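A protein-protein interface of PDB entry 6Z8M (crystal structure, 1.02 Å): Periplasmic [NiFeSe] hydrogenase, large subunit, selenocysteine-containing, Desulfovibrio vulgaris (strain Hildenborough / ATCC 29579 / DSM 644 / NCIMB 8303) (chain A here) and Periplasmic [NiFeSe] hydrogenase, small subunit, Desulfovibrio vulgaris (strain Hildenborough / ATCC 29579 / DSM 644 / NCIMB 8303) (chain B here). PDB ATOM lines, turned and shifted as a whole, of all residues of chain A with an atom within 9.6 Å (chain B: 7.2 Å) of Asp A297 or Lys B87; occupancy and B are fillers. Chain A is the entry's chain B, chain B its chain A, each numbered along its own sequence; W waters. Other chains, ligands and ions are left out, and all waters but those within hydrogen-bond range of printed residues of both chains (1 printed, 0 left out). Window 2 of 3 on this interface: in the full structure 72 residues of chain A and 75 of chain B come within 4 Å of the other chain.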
ATOM      1  N   HIS A  19      32.539  19.843  14.245  1.00  0.00           N
ATOM      2  CA  HIS A  19      31.129  19.893  13.870  1.00  0.00           C
ATOM      3  C   HIS A  19      30.592  18.474  13.738  1.00  0.00           C
ATOM      4  O   HIS A  19      30.904  17.773  12.767  1.00  0.00           O
ATOM      5  CB  HIS A  19      30.982  20.612  12.537  1.00  0.00           C
ATOM      6  CG  HIS A  19      31.528  22.001  12.536  1.00  0.00           C
ATOM      7  ND1 HIS A  19      32.881  22.284  12.514  1.00  0.00           N
ATOM      8  CD2 HIS A  19      30.889  23.191  12.516  1.00  0.00           C
ATOM      9  CE1 HIS A  19      33.044  23.593  12.514  1.00  0.00           C
ATOM     10  NE2 HIS A  19      31.852  24.168  12.507  1.00  0.00           N
ATOM     11  N   GLY A  38      29.832  14.253  10.288  1.00  0.00           N
ATOM     12  CA  GLY A  38      30.812  15.321  10.358  1.00  0.00           C
ATOM     13  C   GLY A  38      30.401  16.395   9.384  1.00  0.00           C
ATOM     14  O   GLY A  38      30.287  16.125   8.181  1.00  0.00           O
ATOM     15  N   GLY A  39      30.148  17.601   9.884  1.00  0.00           N
ATOM     16  CA  GLY A  39      29.407  18.602   9.151  1.00  0.00           C
ATOM     17  C   GLY A  39      30.170  19.726   8.499  1.00  0.00           C
ATOM     18  O   GLY A  39      29.537  20.592   7.893  1.00  0.00           O
ATOM     19  N   MET A  40      31.492  19.755   8.596  1.00  0.00           N
ATOM     20  CA  MET A  40      32.270  20.852   8.038  1.00  0.00           C
ATOM     21  C   MET A  40      33.461  20.322   7.261  1.00  0.00           C
ATOM     22  O   MET A  40      34.255  19.521   7.770  1.00  0.00           O
ATOM     23  CB  MET A  40      32.724  21.807   9.144  1.00  0.00           C
ATOM     24  CG  MET A  40      33.456  23.056   8.646  1.00  0.00           C
ATOM     25  SD  MET A  40      35.217  22.796   8.329  1.00  0.00           S
ATOM     26  CE  MET A  40      35.847  22.655  10.000  1.00  0.00           C
ATOM     27  N   TYR A  41      33.589  20.794   6.030  1.00  0.00           N
ATOM     28  CA  TYR A  41      34.624  20.346   5.116  1.00  0.00           C
ATOM     29  C   TYR A  41      35.465  21.523   4.652  1.00  0.00           C
ATOM     30  O   TYR A  41      34.937  22.585   4.314  1.00  0.00           O
ATOM     31  CB  TYR A  41      33.982  19.671   3.903  1.00  0.00           C
ATOM     32  CG  TYR A  41      34.926  19.251   2.809  1.00  0.00           C
ATOM     33  CD1 TYR A  41      35.625  18.059   2.882  1.00  0.00           C
ATOM     34  CD2 TYR A  41      35.105  20.044   1.677  1.00  0.00           C
ATOM     35  CE1 TYR A  41      36.494  17.674   1.873  1.00  0.00           C
ATOM     36  CE2 TYR A  41      35.954  19.664   0.651  1.00  0.00           C
ATOM     37  CZ  TYR A  41      36.646  18.474   0.756  1.00  0.00           C
ATOM     38  OH  TYR A  41      37.496  18.073  -0.246  1.00  0.00           O
ATOM     39  N   ARG A  42      36.766  21.290   4.565  1.00  0.00           N
ATOM     40  CA  ARG A  42      37.704  22.256   3.991  1.00  0.00           C
ATOM     41  C   ARG A  42      38.483  21.724   2.799  1.00  0.00           C
ATOM     42  O   ARG A  42      38.739  22.481   1.865  1.00  0.00           O
ATOM     43  CB  ARG A  42      38.658  22.771   5.076  1.00  0.00           C
ATOM     44  CG  ARG A  42      37.928  23.693   6.059  1.00  0.00           C
ATOM     45  CD  ARG A  42      38.639  23.889   7.387  1.00  0.00           C
ATOM     46  NE  ARG A  42      38.805  22.613   8.060  1.00  0.00           N
ATOM     47  CZ  ARG A  42      39.756  22.342   8.945  1.00  0.00           C
ATOM     48  NH1 ARG A  42      40.587  23.278   9.367  1.00  0.00           N
ATOM     49  NH2 ARG A  42      39.868  21.105   9.422  1.00  0.00           N
ATOM     50  N   LYS A 274      30.358   5.322   0.329  1.00  0.00           N
ATOM     51  CA  LYS A 274      28.935   5.260  -0.003  1.00  0.00           C
ATOM     52  C   LYS A 274      28.097   6.216   0.843  1.00  0.00           C
ATOM     53  O   LYS A 274      27.173   6.863   0.333  1.00  0.00           O
ATOM     54  CB  LYS A 274      28.407   3.836   0.157  1.00  0.00           C
ATOM     55  CG  LYS A 274      26.900   3.701  -0.072  1.00  0.00           C
ATOM     56  CD  LYS A 274      26.481   2.246  -0.048  1.00  0.00           C
ATOM     57  CE  LYS A 274      24.980   2.085  -0.220  1.00  0.00           C
ATOM     58  NZ  LYS A 274      24.589   0.660  -0.353  1.00  0.00           N
ATOM     59  N   SER A 276      29.284   8.800   2.568  1.00  0.00           N
ATOM     60  CA  SER A 276      30.039  10.030   2.731  1.00  0.00           C
ATOM     61  C   SER A 276      29.837  10.911   1.500  1.00  0.00           C
ATOM     62  O   SER A 276      29.586  10.413   0.400  1.00  0.00           O
ATOM     63  CB  SER A 276      31.524   9.703   2.902  1.00  0.00           C
ATOM     64  OG  SER A 276      31.731   8.715   3.881  1.00  0.00           O
ATOM     65  N   TRP A 277      29.970  12.226   1.688  1.00  0.00           N
ATOM     66  CA  TRP A 277      29.713  13.198   0.624  1.00  0.00           C
ATOM     67  C   TRP A 277      30.919  13.356  -0.308  1.00  0.00           C
ATOM     68  O   TRP A 277      31.512  14.427  -0.429  1.00  0.00           O
ATOM     69  CB  TRP A 277      29.283  14.534   1.212  1.00  0.00           C
ATOM     70  CG  TRP A 277      27.899  14.530   1.777  1.00  0.00           C
ATOM     71  CD1 TRP A 277      26.755  14.163   1.134  1.00  0.00           C
ATOM     72  CD2 TRP A 277      27.506  14.928   3.097  1.00  0.00           C
ATOM     73  NE1 TRP A 277      25.673  14.307   1.971  1.00  0.00           N
ATOM     74  CE2 TRP A 277      26.105  14.778   3.181  1.00  0.00           C
ATOM     75  CE3 TRP A 277      28.199  15.426   4.205  1.00  0.00           C
ATOM     76  CZ2 TRP A 277      25.390  15.083   4.334  1.00  0.00           C
ATOM     77  CZ3 TRP A 277      27.491  15.734   5.346  1.00  0.00           C
ATOM     78  CH2 TRP A 277      26.094  15.561   5.406  1.00  0.00           C
ATOM     79  N   PHE A 278      31.268  12.250  -0.967  1.00  0.00           N
ATOM     80  CA  PHE A 278      32.321  12.201  -1.973  1.00  0.00           C
ATOM     81  C   PHE A 278      31.854  11.383  -3.167  1.00  0.00           C
ATOM     82  O   PHE A 278      30.966  10.537  -3.055  1.00  0.00           O
ATOM     83  CB  PHE A 278      33.610  11.621  -1.386  1.00  0.00           C
ATOM     84  CG  PHE A 278      34.113  12.429  -0.242  1.00  0.00           C
ATOM     85  CD1 PHE A 278      34.807  13.591  -0.474  1.00  0.00           C
ATOM     86  CD2 PHE A 278      33.814  12.092   1.061  1.00  0.00           C
ATOM     87  CE1 PHE A 278      35.218  14.389   0.565  1.00  0.00           C
ATOM     88  CE2 PHE A 278      34.229  12.888   2.108  1.00  0.00           C
ATOM     89  CZ  PHE A 278      34.927  14.032   1.858  1.00  0.00           C
ATOM     90  N   ALA A 279      32.462  11.647  -4.316  1.00  0.00           N
ATOM     91  CA  ALA A 279      32.045  11.002  -5.556  1.00  0.00           C
ATOM     92  C   ALA A 279      32.119   9.484  -5.427  1.00  0.00           C
ATOM     93  O   ALA A 279      33.103   8.925  -4.933  1.00  0.00           O
ATOM     94  CB  ALA A 279      32.937  11.475  -6.697  1.00  0.00           C
ATOM     95  N   GLU A 280      31.077   8.811  -5.924  1.00  0.00           N
ATOM     96  CA  GLU A 280      30.966   7.359  -5.768  1.00  0.00           C
ATOM     97  C   GLU A 280      32.168   6.627  -6.347  1.00  0.00           C
ATOM     98  O   GLU A 280      32.581   5.589  -5.817  1.00  0.00           O
ATOM     99  CB  GLU A 280      29.706   6.834  -6.463  1.00  0.00           C
ATOM    100  CG  GLU A 280      28.403   7.453  -6.028  1.00  0.00           C
ATOM    101  CD  GLU A 280      27.178   6.638  -6.418  1.00  0.00           C
ATOM    102  OE1 GLU A 280      27.289   5.745  -7.289  1.00  0.00           O
ATOM    103  OE2 GLU A 280      26.094   6.907  -5.852  1.00  0.00           O
ATOM    104  N   ILE A 293      37.071  14.021  -3.721  1.00  0.00           N
ATOM    105  CA  ILE A 293      36.206  14.672  -4.692  1.00  0.00           C
ATOM    106  C   ILE A 293      34.869  14.907  -4.004  1.00  0.00           C
ATOM    107  O   ILE A 293      34.036  13.994  -3.941  1.00  0.00           O
ATOM    108  CB  ILE A 293      36.050  13.828  -5.966  1.00  0.00           C
ATOM    109  CG1 ILE A 293      37.426  13.525  -6.567  1.00  0.00           C
ATOM    110  CG2 ILE A 293      35.148  14.558  -6.959  1.00  0.00           C
ATOM    111  CD1 ILE A 293      37.362  12.706  -7.840  1.00  0.00           C
ATOM    112  N   PRO A 294      34.632  16.089  -3.447  1.00  0.00           N
ATOM    113  CA  PRO A 294      33.408  16.295  -2.671  1.00  0.00           C
ATOM    114  C   PRO A 294      32.155  16.170  -3.518  1.00  0.00           C
ATOM    115  O   PRO A 294      32.125  16.513  -4.704  1.00  0.00           O
ATOM    116  CB  PRO A 294      33.568  17.707  -2.084  1.00  0.00           C
ATOM    117  CG  PRO A 294      34.702  18.319  -2.753  1.00  0.00           C
ATOM    118  CD  PRO A 294      35.520  17.259  -3.419  1.00  0.00           C
ATOM    119  N   ALA A 295      31.117  15.639  -2.885  1.00  0.00           N
ATOM    120  CA  ALA A 295      29.809  15.456  -3.508  1.00  0.00           C
ATOM    121  C   ALA A 295      28.760  15.765  -2.457  1.00  0.00           C
ATOM    122  O   ALA A 295      28.093  14.869  -1.925  1.00  0.00           O
ATOM    123  CB  ALA A 295      29.658  14.035  -4.045  1.00  0.00           C
ATOM    124  N   PRO A 296      28.590  17.046  -2.127  1.00  0.00           N
ATOM    125  CA  PRO A 296      27.740  17.416  -0.988  1.00  0.00           C
ATOM    126  C   PRO A 296      26.271  17.157  -1.202  1.00  0.00           C
ATOM    127  O   PRO A 296      25.519  17.209  -0.226  1.00  0.00           O
ATOM    128  CB  PRO A 296      28.008  18.917  -0.819  1.00  0.00           C
ATOM    129  CG  PRO A 296      28.420  19.369  -2.180  1.00  0.00           C
ATOM    130  CD  PRO A 296      29.222  18.225  -2.745  1.00  0.00           C
ATOM    131  N   ASP A 297      25.836  16.899  -2.431  1.00  0.00           N
ATOM    132  CA  ASP A 297      24.442  16.608  -2.723  1.00  0.00           C
ATOM    133  C   ASP A 297      24.181  15.127  -2.964  1.00  0.00           C
ATOM    134  O   ASP A 297      23.073  14.760  -3.360  1.00  0.00           O
ATOM    135  CB  ASP A 297      23.985  17.428  -3.934  1.00  0.00           C
ATOM    136  CG  ASP A 297      24.078  18.924  -3.688  1.00  0.00           C
ATOM    137  OD1 ASP A 297      23.685  19.366  -2.595  1.00  0.00           O
ATOM    138  OD2 ASP A 297      24.557  19.660  -4.576  1.00  0.00           O
ATOM    139  N   LYS A 298      25.160  14.260  -2.724  1.00  0.00           N
ATOM    140  CA  LYS A 298      24.970  12.853  -3.054  1.00  0.00           C
ATOM    141  C   LYS A 298      23.912  12.215  -2.156  1.00  0.00           C
ATOM    142  O   LYS A 298      24.007  12.261  -0.925  1.00  0.00           O
ATOM    143  CB  LYS A 298      26.284  12.082  -2.955  1.00  0.00           C
ATOM    144  CG  LYS A 298      26.141  10.644  -3.482  1.00  0.00           C
ATOM    145  CD  LYS A 298      27.436   9.861  -3.419  1.00  0.00           C
ATOM    146  CE  LYS A 298      27.819   9.530  -2.003  1.00  0.00           C
ATOM    147  NZ  LYS A 298      29.081   8.746  -1.944  1.00  0.00           N
ATOM    148  N   ALA A 299      22.917  11.589  -2.780  1.00  0.00           N
ATOM    149  CA  ALA A 299      21.820  10.984  -2.037  1.00  0.00           C
ATOM    150  C   ALA A 299      22.328   9.862  -1.148  1.00  0.00           C
ATOM    151  O   ALA A 299      23.215   9.094  -1.534  1.00  0.00           O
ATOM    152  CB  ALA A 299      20.797  10.403  -3.013  1.00  0.00           C
ATOM    153  N   GLY A 300      21.750   9.768   0.048  1.00  0.00           N
ATOM    154  CA  GLY A 300      22.053   8.702   0.978  1.00  0.00           C
ATOM    155  C   GLY A 300      23.263   8.932   1.852  1.00  0.00           C
ATOM    156  O   GLY A 300      23.375   8.295   2.900  1.00  0.00           O
ATOM    157  N   ALA A 301      24.166   9.821   1.462  1.00  0.00           N
ATOM    158  CA  ALA A 301      25.336  10.120   2.276  1.00  0.00           C
ATOM    159  C   ALA A 301      24.951  11.013   3.450  1.00  0.00           C
ATOM    160  O   ALA A 301      23.973  11.767   3.392  1.00  0.00           O
ATOM    161  CB  ALA A 301      26.393  10.821   1.427  1.00  0.00           C
ATOM    162  N   TYR A 302      25.734  10.931   4.527  1.00  0.00           N
ATOM    163  CA  TYR A 302      25.396  11.717   5.706  1.00  0.00           C
ATOM    164  C   TYR A 302      26.600  12.267   6.458  1.00  0.00           C
ATOM    165  O   TYR A 302      26.441  12.714   7.604  1.00  0.00           O
ATOM    166  CB  TYR A 302      24.462  10.949   6.652  1.00  0.00           C
ATOM    167  CG  TYR A 302      24.991   9.659   7.276  1.00  0.00           C
ATOM    168  CD1 TYR A 302      25.736   9.686   8.446  1.00  0.00           C
ATOM    169  CD2 TYR A 302      24.691   8.415   6.733  1.00  0.00           C
ATOM    170  CE1 TYR A 302      26.192   8.534   9.040  1.00  0.00           C
ATOM    171  CE2 TYR A 302      25.138   7.245   7.330  1.00  0.00           C
ATOM    172  CZ  TYR A 302      25.893   7.303   8.475  1.00  0.00           C
ATOM    173  OH  TYR A 302      26.322   6.127   9.058  1.00  0.00           O
ATOM    174  N   SER A 303      27.784  12.302   5.844  1.00  0.00           N
ATOM    175  CA  SER A 303      28.950  12.806   6.554  1.00  0.00           C
ATOM    176  C   SER A 303      30.032  13.213   5.570  1.00  0.00           C
ATOM    177  O   SER A 303      30.143  12.630   4.490  1.00  0.00           O
ATOM    178  CB  SER A 303      29.502  11.701   7.444  1.00  0.00           C
ATOM    179  OG  SER A 303      30.518  12.246   8.250  1.00  0.00           O
ATOM    180  N   PHE A 304      30.857  14.189   5.972  1.00  0.00           N
ATOM    181  CA  PHE A 304      32.082  14.498   5.241  1.00  0.00           C
ATOM    182  C   PHE A 304      33.261  13.647   5.695  1.00  0.00           C
ATOM    183  O   PHE A 304      34.373  13.821   5.184  1.00  0.00           O
ATOM    184  CB  PHE A 304      32.432  15.983   5.359  1.00  0.00           C
ATOM    185  CG  PHE A 304      31.540  16.896   4.556  1.00  0.00           C
ATOM    186  CD1 PHE A 304      31.549  16.862   3.168  1.00  0.00           C
ATOM    187  CD2 PHE A 304      30.723  17.826   5.184  1.00  0.00           C
ATOM    188  CE1 PHE A 304      30.738  17.708   2.426  1.00  0.00           C
ATOM    189  CE2 PHE A 304      29.923  18.687   4.458  1.00  0.00           C
ATOM    190  CZ  PHE A 304      29.918  18.623   3.074  1.00  0.00           C
ATOM    191  N   VAL A 483      37.516  15.134   9.094  1.00  0.00           N
ATOM    192  CA  VAL A 483      37.120  15.557   7.762  1.00  0.00           C
ATOM    193  C   VAL A 483      38.272  16.175   6.983  1.00  0.00           C
ATOM    194  O   VAL A 483      38.441  15.897   5.794  1.00  0.00           O
ATOM    195  CB  VAL A 483      35.932  16.540   7.825  1.00  0.00           C
ATOM    196  CG1 VAL A 483      35.598  17.004   6.430  1.00  0.00           C
ATOM    197  CG2 VAL A 483      34.714  15.898   8.495  1.00  0.00           C
ATOM    198  N   PRO B  81      31.741  29.132   4.188  1.00  0.00           N
ATOM    199  CA  PRO B  81      31.712  28.603   2.822  1.00  0.00           C
ATOM    200  C   PRO B  81      30.350  28.777   2.184  1.00  0.00           C
ATOM    201  O   PRO B  81      29.334  28.342   2.734  1.00  0.00           O
ATOM    202  CB  PRO B  81      32.075  27.129   3.016  1.00  0.00           C
ATOM    203  CG  PRO B  81      31.543  26.794   4.393  1.00  0.00           C
ATOM    204  CD  PRO B  81      31.616  28.068   5.201  1.00  0.00           C
ATOM    205  N   VAL B  82      30.314  29.406   1.008  1.00  0.00           N
ATOM    206  CA  VAL B  82      29.050  29.720   0.356  1.00  0.00           C
ATOM    207  C   VAL B  82      28.657  28.726  -0.725  1.00  0.00           C
ATOM    208  O   VAL B  82      27.505  28.761  -1.176  1.00  0.00           O
ATOM    209  CB  VAL B  82      29.033  31.159  -0.208  1.00  0.00           C
ATOM    210  CG1 VAL B  82      29.257  32.166   0.911  1.00  0.00           C
ATOM    211  CG2 VAL B  82      30.051  31.340  -1.323  1.00  0.00           C
ATOM    212  N   GLU B  83      29.565  27.868  -1.173  1.00  0.00           N
ATOM    213  CA  GLU B  83      29.215  26.946  -2.246  1.00  0.00           C
ATOM    214  C   GLU B  83      28.213  25.906  -1.759  1.00  0.00           C
ATOM    215  O   GLU B  83      28.042  25.667  -0.568  1.00  0.00           O
ATOM    216  CB  GLU B  83      30.448  26.228  -2.777  1.00  0.00           C
ATOM    217  CG  GLU B  83      31.390  27.115  -3.573  1.00  0.00           C
ATOM    218  CD  GLU B  83      30.838  27.518  -4.928  1.00  0.00           C
ATOM    219  OE1 GLU B  83      30.033  26.760  -5.491  1.00  0.00           O
ATOM    220  OE2 GLU B  83      31.224  28.599  -5.426  1.00  0.00           O
ATOM    221  N   ALA B  84      27.529  25.287  -2.708  1.00  0.00           N
ATOM    222  CA  ALA B  84      26.601  24.203  -2.398  1.00  0.00           C
ATOM    223  C   ALA B  84      25.573  24.622  -1.354  1.00  0.00           C
ATOM    224  O   ALA B  84      25.233  23.862  -0.445  1.00  0.00           O
ATOM    225  CB  ALA B  84      27.343  22.936  -1.962  1.00  0.00           C
ATOM    226  N   ASP B  85      25.060  25.843  -1.496  1.00  0.00           N
ATOM    227  CA  ASP B  85      24.008  26.354  -0.622  1.00  0.00           C
ATOM    228  C   ASP B  85      24.390  26.253   0.854  1.00  0.00           C
ATOM    229  O   ASP B  85      23.546  26.010   1.715  1.00  0.00           O
ATOM    230  CB  ASP B  85      22.681  25.643  -0.896  1.00  0.00           C
ATOM    231  CG  ASP B  85      21.498  26.326  -0.242  1.00  0.00           C
ATOM    232  OD1 ASP B  85      21.461  27.571  -0.212  1.00  0.00           O
ATOM    233  OD2 ASP B  85      20.582  25.606   0.212  1.00  0.00           O
ATOM    234  N   GLY B  86      25.672  26.456   1.152  1.00  0.00           N
ATOM    235  CA  GLY B  86      26.139  26.496   2.521  1.00  0.00           C
ATOM    236  C   GLY B  86      26.480  25.151   3.124  1.00  0.00           C
ATOM    237  O   GLY B  86      26.891  25.098   4.293  1.00  0.00           O
ATOM    238  N   LYS B  87      26.304  24.062   2.377  1.00  0.00           N
ATOM    239  CA  LYS B  87      26.372  22.712   2.936  1.00  0.00           C
ATOM    240  C   LYS B  87      27.750  22.311   3.438  1.00  0.00           C
ATOM    241  O   LYS B  87      27.860  21.302   4.152  1.00  0.00           O
ATOM    242  CB  LYS B  87      25.902  21.685   1.900  1.00  0.00           C
ATOM    243  CG  LYS B  87      24.413  21.680   1.666  1.00  0.00           C
ATOM    244  CD  LYS B  87      24.007  20.520   0.761  1.00  0.00           C
ATOM    245  CE  LYS B  87      22.517  20.501   0.518  1.00  0.00           C
ATOM    246  NZ  LYS B  87      22.126  19.315  -0.276  1.00  0.00           N
ATOM    247  N   TYR B  88      28.805  23.033   3.076  1.00  0.00           N
ATOM    248  CA  TYR B  88      30.119  22.647   3.557  1.00  0.00           C
ATOM    249  C   TYR B  88      30.375  23.064   5.000  1.00  0.00           C
ATOM    250  O   TYR B  88      31.444  22.755   5.529  1.00  0.00           O
ATOM    251  CB  TYR B  88      31.213  23.199   2.647  1.00  0.00           C
ATOM    252  CG  TYR B  88      31.286  22.538   1.287  1.00  0.00           C
ATOM    253  CD1 TYR B  88      31.588  21.197   1.162  1.00  0.00           C
ATOM    254  CD2 TYR B  88      31.103  23.269   0.122  1.00  0.00           C
ATOM    255  CE1 TYR B  88      31.688  20.595  -0.081  1.00  0.00           C
ATOM    256  CE2 TYR B  88      31.199  22.675  -1.134  1.00  0.00           C
ATOM    257  CZ  TYR B  88      31.488  21.328  -1.221  1.00  0.00           C
ATOM    258  OH  TYR B  88      31.607  20.701  -2.429  1.00  0.00           O
ATOM    259  N   CYS B  89      29.431  23.733   5.665  1.00  0.00           N
ATOM    260  CA  CYS B  89      29.555  23.935   7.108  1.00  0.00           C
ATOM    261  C   CYS B  89      28.171  24.008   7.738  1.00  0.00           C
ATOM    262  O   CYS B  89      27.497  25.029   7.622  1.00  0.00           O
ATOM    263  CB  CYS B  89      30.332  25.201   7.412  1.00  0.00           C
ATOM    264  SG  CYS B  89      30.614  25.430   9.174  1.00  0.00           S
ATOM    265  N   ILE B  90      27.776  22.933   8.416  1.00  0.00           N
ATOM    266  CA  ILE B  90      26.532  22.864   9.175  1.00  0.00           C
ATOM    267  C   ILE B  90      26.904  22.962  10.646  1.00  0.00           C
ATOM    268  O   ILE B  90      27.712  22.165  11.139  1.00  0.00           O
ATOM    269  CB  ILE B  90      25.765  21.568   8.878  1.00  0.00           C
ATOM    270  CG1 ILE B  90      25.373  21.508   7.394  1.00  0.00           C
ATOM    271  CG2 ILE B  90      24.546  21.481   9.775  1.00  0.00           C
ATOM    272  CD1 ILE B  90      24.537  22.684   6.909  1.00  0.00           C
ATOM    273  N   GLU B  98      18.423  21.959   9.471  1.00  0.00           N
ATOM    274  CA  GLU B  98      19.848  22.189   9.626  1.00  0.00           C
ATOM    275  C   GLU B  98      20.147  23.678   9.481  1.00  0.00           C
ATOM    276  O   GLU B  98      19.423  24.419   8.809  1.00  0.00           O
ATOM    277  CB  GLU B  98      20.633  21.354   8.611  1.00  0.00           C
ATOM    278  CG  GLU B  98      20.482  21.781   7.190  1.00  0.00           C
ATOM    279  CD  GLU B  98      21.080  20.788   6.208  1.00  0.00           C
ATOM    280  OE1 GLU B  98      21.762  19.836   6.644  1.00  0.00           O
ATOM    281  OE2 GLU B  98      20.864  20.956   4.993  1.00  0.00           O
ATOM    282  N   SER B 100      23.225  26.142   8.470  1.00  0.00           N
ATOM    283  CA  SER B 100      24.563  26.299   7.927  1.00  0.00           C
ATOM    284  C   SER B 100      25.229  27.530   8.542  1.00  0.00           C
ATOM    285  O   SER B 100      24.587  28.365   9.177  1.00  0.00           O
ATOM    286  CB  SER B 100      24.487  26.465   6.417  1.00  0.00           C
ATOM    287  OG  SER B 100      23.910  27.722   6.099  1.00  0.00           O
ATOM    288  N   MET B 101      26.540  27.634   8.338  1.00  0.00           N
ATOM    289  CA  MET B 101      27.250  28.834   8.759  1.00  0.00           C
ATOM    290  C   MET B 101      26.688  30.065   8.060  1.00  0.00           C
ATOM    291  O   MET B 101      26.512  31.117   8.685  1.00  0.00           O
ATOM    292  CB  MET B 101      28.741  28.680   8.473  1.00  0.00           C
ATOM    293  CG  MET B 101      29.585  29.777   9.091  1.00  0.00           C
ATOM    294  SD  MET B 101      29.547  29.719  10.891  1.00  0.00           S
ATOM    295  CE  MET B 101      30.670  31.036  11.275  1.00  0.00           C
ATOM    296  N   VAL B 102      26.376  29.940   6.767  1.00  0.00           N
ATOM    297  CA  VAL B 102      25.718  31.013   6.020  1.00  0.00           C
ATOM    298  C   VAL B 102      24.442  31.443   6.730  1.00  0.00           C
ATOM    299  O   VAL B 102      24.198  32.637   6.949  1.00  0.00           O
ATOM    300  CB  VAL B 102      25.436  30.548   4.579  1.00  0.00           C
ATOM    301  CG1 VAL B 102      24.409  31.452   3.896  1.00  0.00           C
ATOM    302  CG2 VAL B 102      26.732  30.474   3.786  1.00  0.00           C
HETATM  303  O   HOH W   1      22.846  16.761   0.863  1.00  0.00           O
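The side-chain amino group (NZ) of Lys B87 lies within salt-bridge range of the side-chain carboxylate (OD1) of Asp A297 (2.8 Å).
The backbone carbonyl oxygen of Tyr B88 is in hydrogen-bond range of the backbone NH of Tyr A41 (2.9 Å).
A ring nitrogen (NE2) of His A19 lies within hydrogen-bond range of the side-chain sulfur (SG) of Cys B89, at 3.8 Å.
O of Gly A39 lies within hydrogen-bond range of N of Ile B90 (3.0 Å).
N of Met B101 is in hydrogen-bond range of O of Cys B89 (2.9 Å).
The backbone carbonyl oxygen (O) of His A19 is in hydrogen-bond range of the backbone NH (N) of Gly A39 (3.0 Å).
O of Gly A38 sits at hydrogen-bond distance from N of Phe A304 (3.0 Å).
The guanidinium group (NE) of Arg A42 sits close to the side-chain sulfur (SD) of Met A40.
Ile B90 touches His A19 (O to CD2, 3.6 Å).
Tyr B88 touches Gly A39 (O to O, 3.7 Å).
Gly A39 touches Cys B89.
O of Tyr B88 touches CA of Met A40, at 3.3 Å.
CG of Met A40 touches SG of Cys B89, at 3.7 Å.
Pro A294 touches Tyr B88 (CB to OH, 3.6 Å).
Pro A296 touches Lys B87.
Pro A296 touches Tyr B88 (CD to OH, 3.5 Å).
Phe A304 touches Lys B87.
Phe A304 touches Tyr B88.
Asp A297 touches one residue of chain B.
Of chain A, only Pro A296, Asp A297 and Phe A304 come within 4 Å of Lys B87.
Of chain A, only Pro A296 comes within 4 Å of Ala B84.
No residue of chain A comes within 4 Å of Gly B86.
Printed residues of chain B within 4 Å of Pro A296: Ala B84 (3.7 Å), Lys B87 (3.8 Å) and Tyr B88 (3.5 Å).
Printed residues of chain A within 4 Å of Tyr B88: Gly A39, Met A40, Tyr A41, Pro A294, Pro A296 and Phe A304.
Hydrophobic or aromatic side chains of chain A within 4 Å of the printed part of chain B: His A19, Met A40, Tyr A41, Pro A294, Pro A296 and Phe A304.
Of the 14 printed residues of chain B, 5 touch a printed residue of chain A.
Printed residues of chain B that touch a printed residue of chain A: Ala B84, Lys B87, Tyr B88, Cys B89 and Ile B90.
Hydrophobic or aromatic side chains of chain B that line the printed part of chain A: Ala B84 and Tyr B88.
Water W1 lies within hydrogen-bond range of the side-chain amino group (NZ) of Lys B87 and the backbone carbonyl oxygen (O) of Pro A296.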
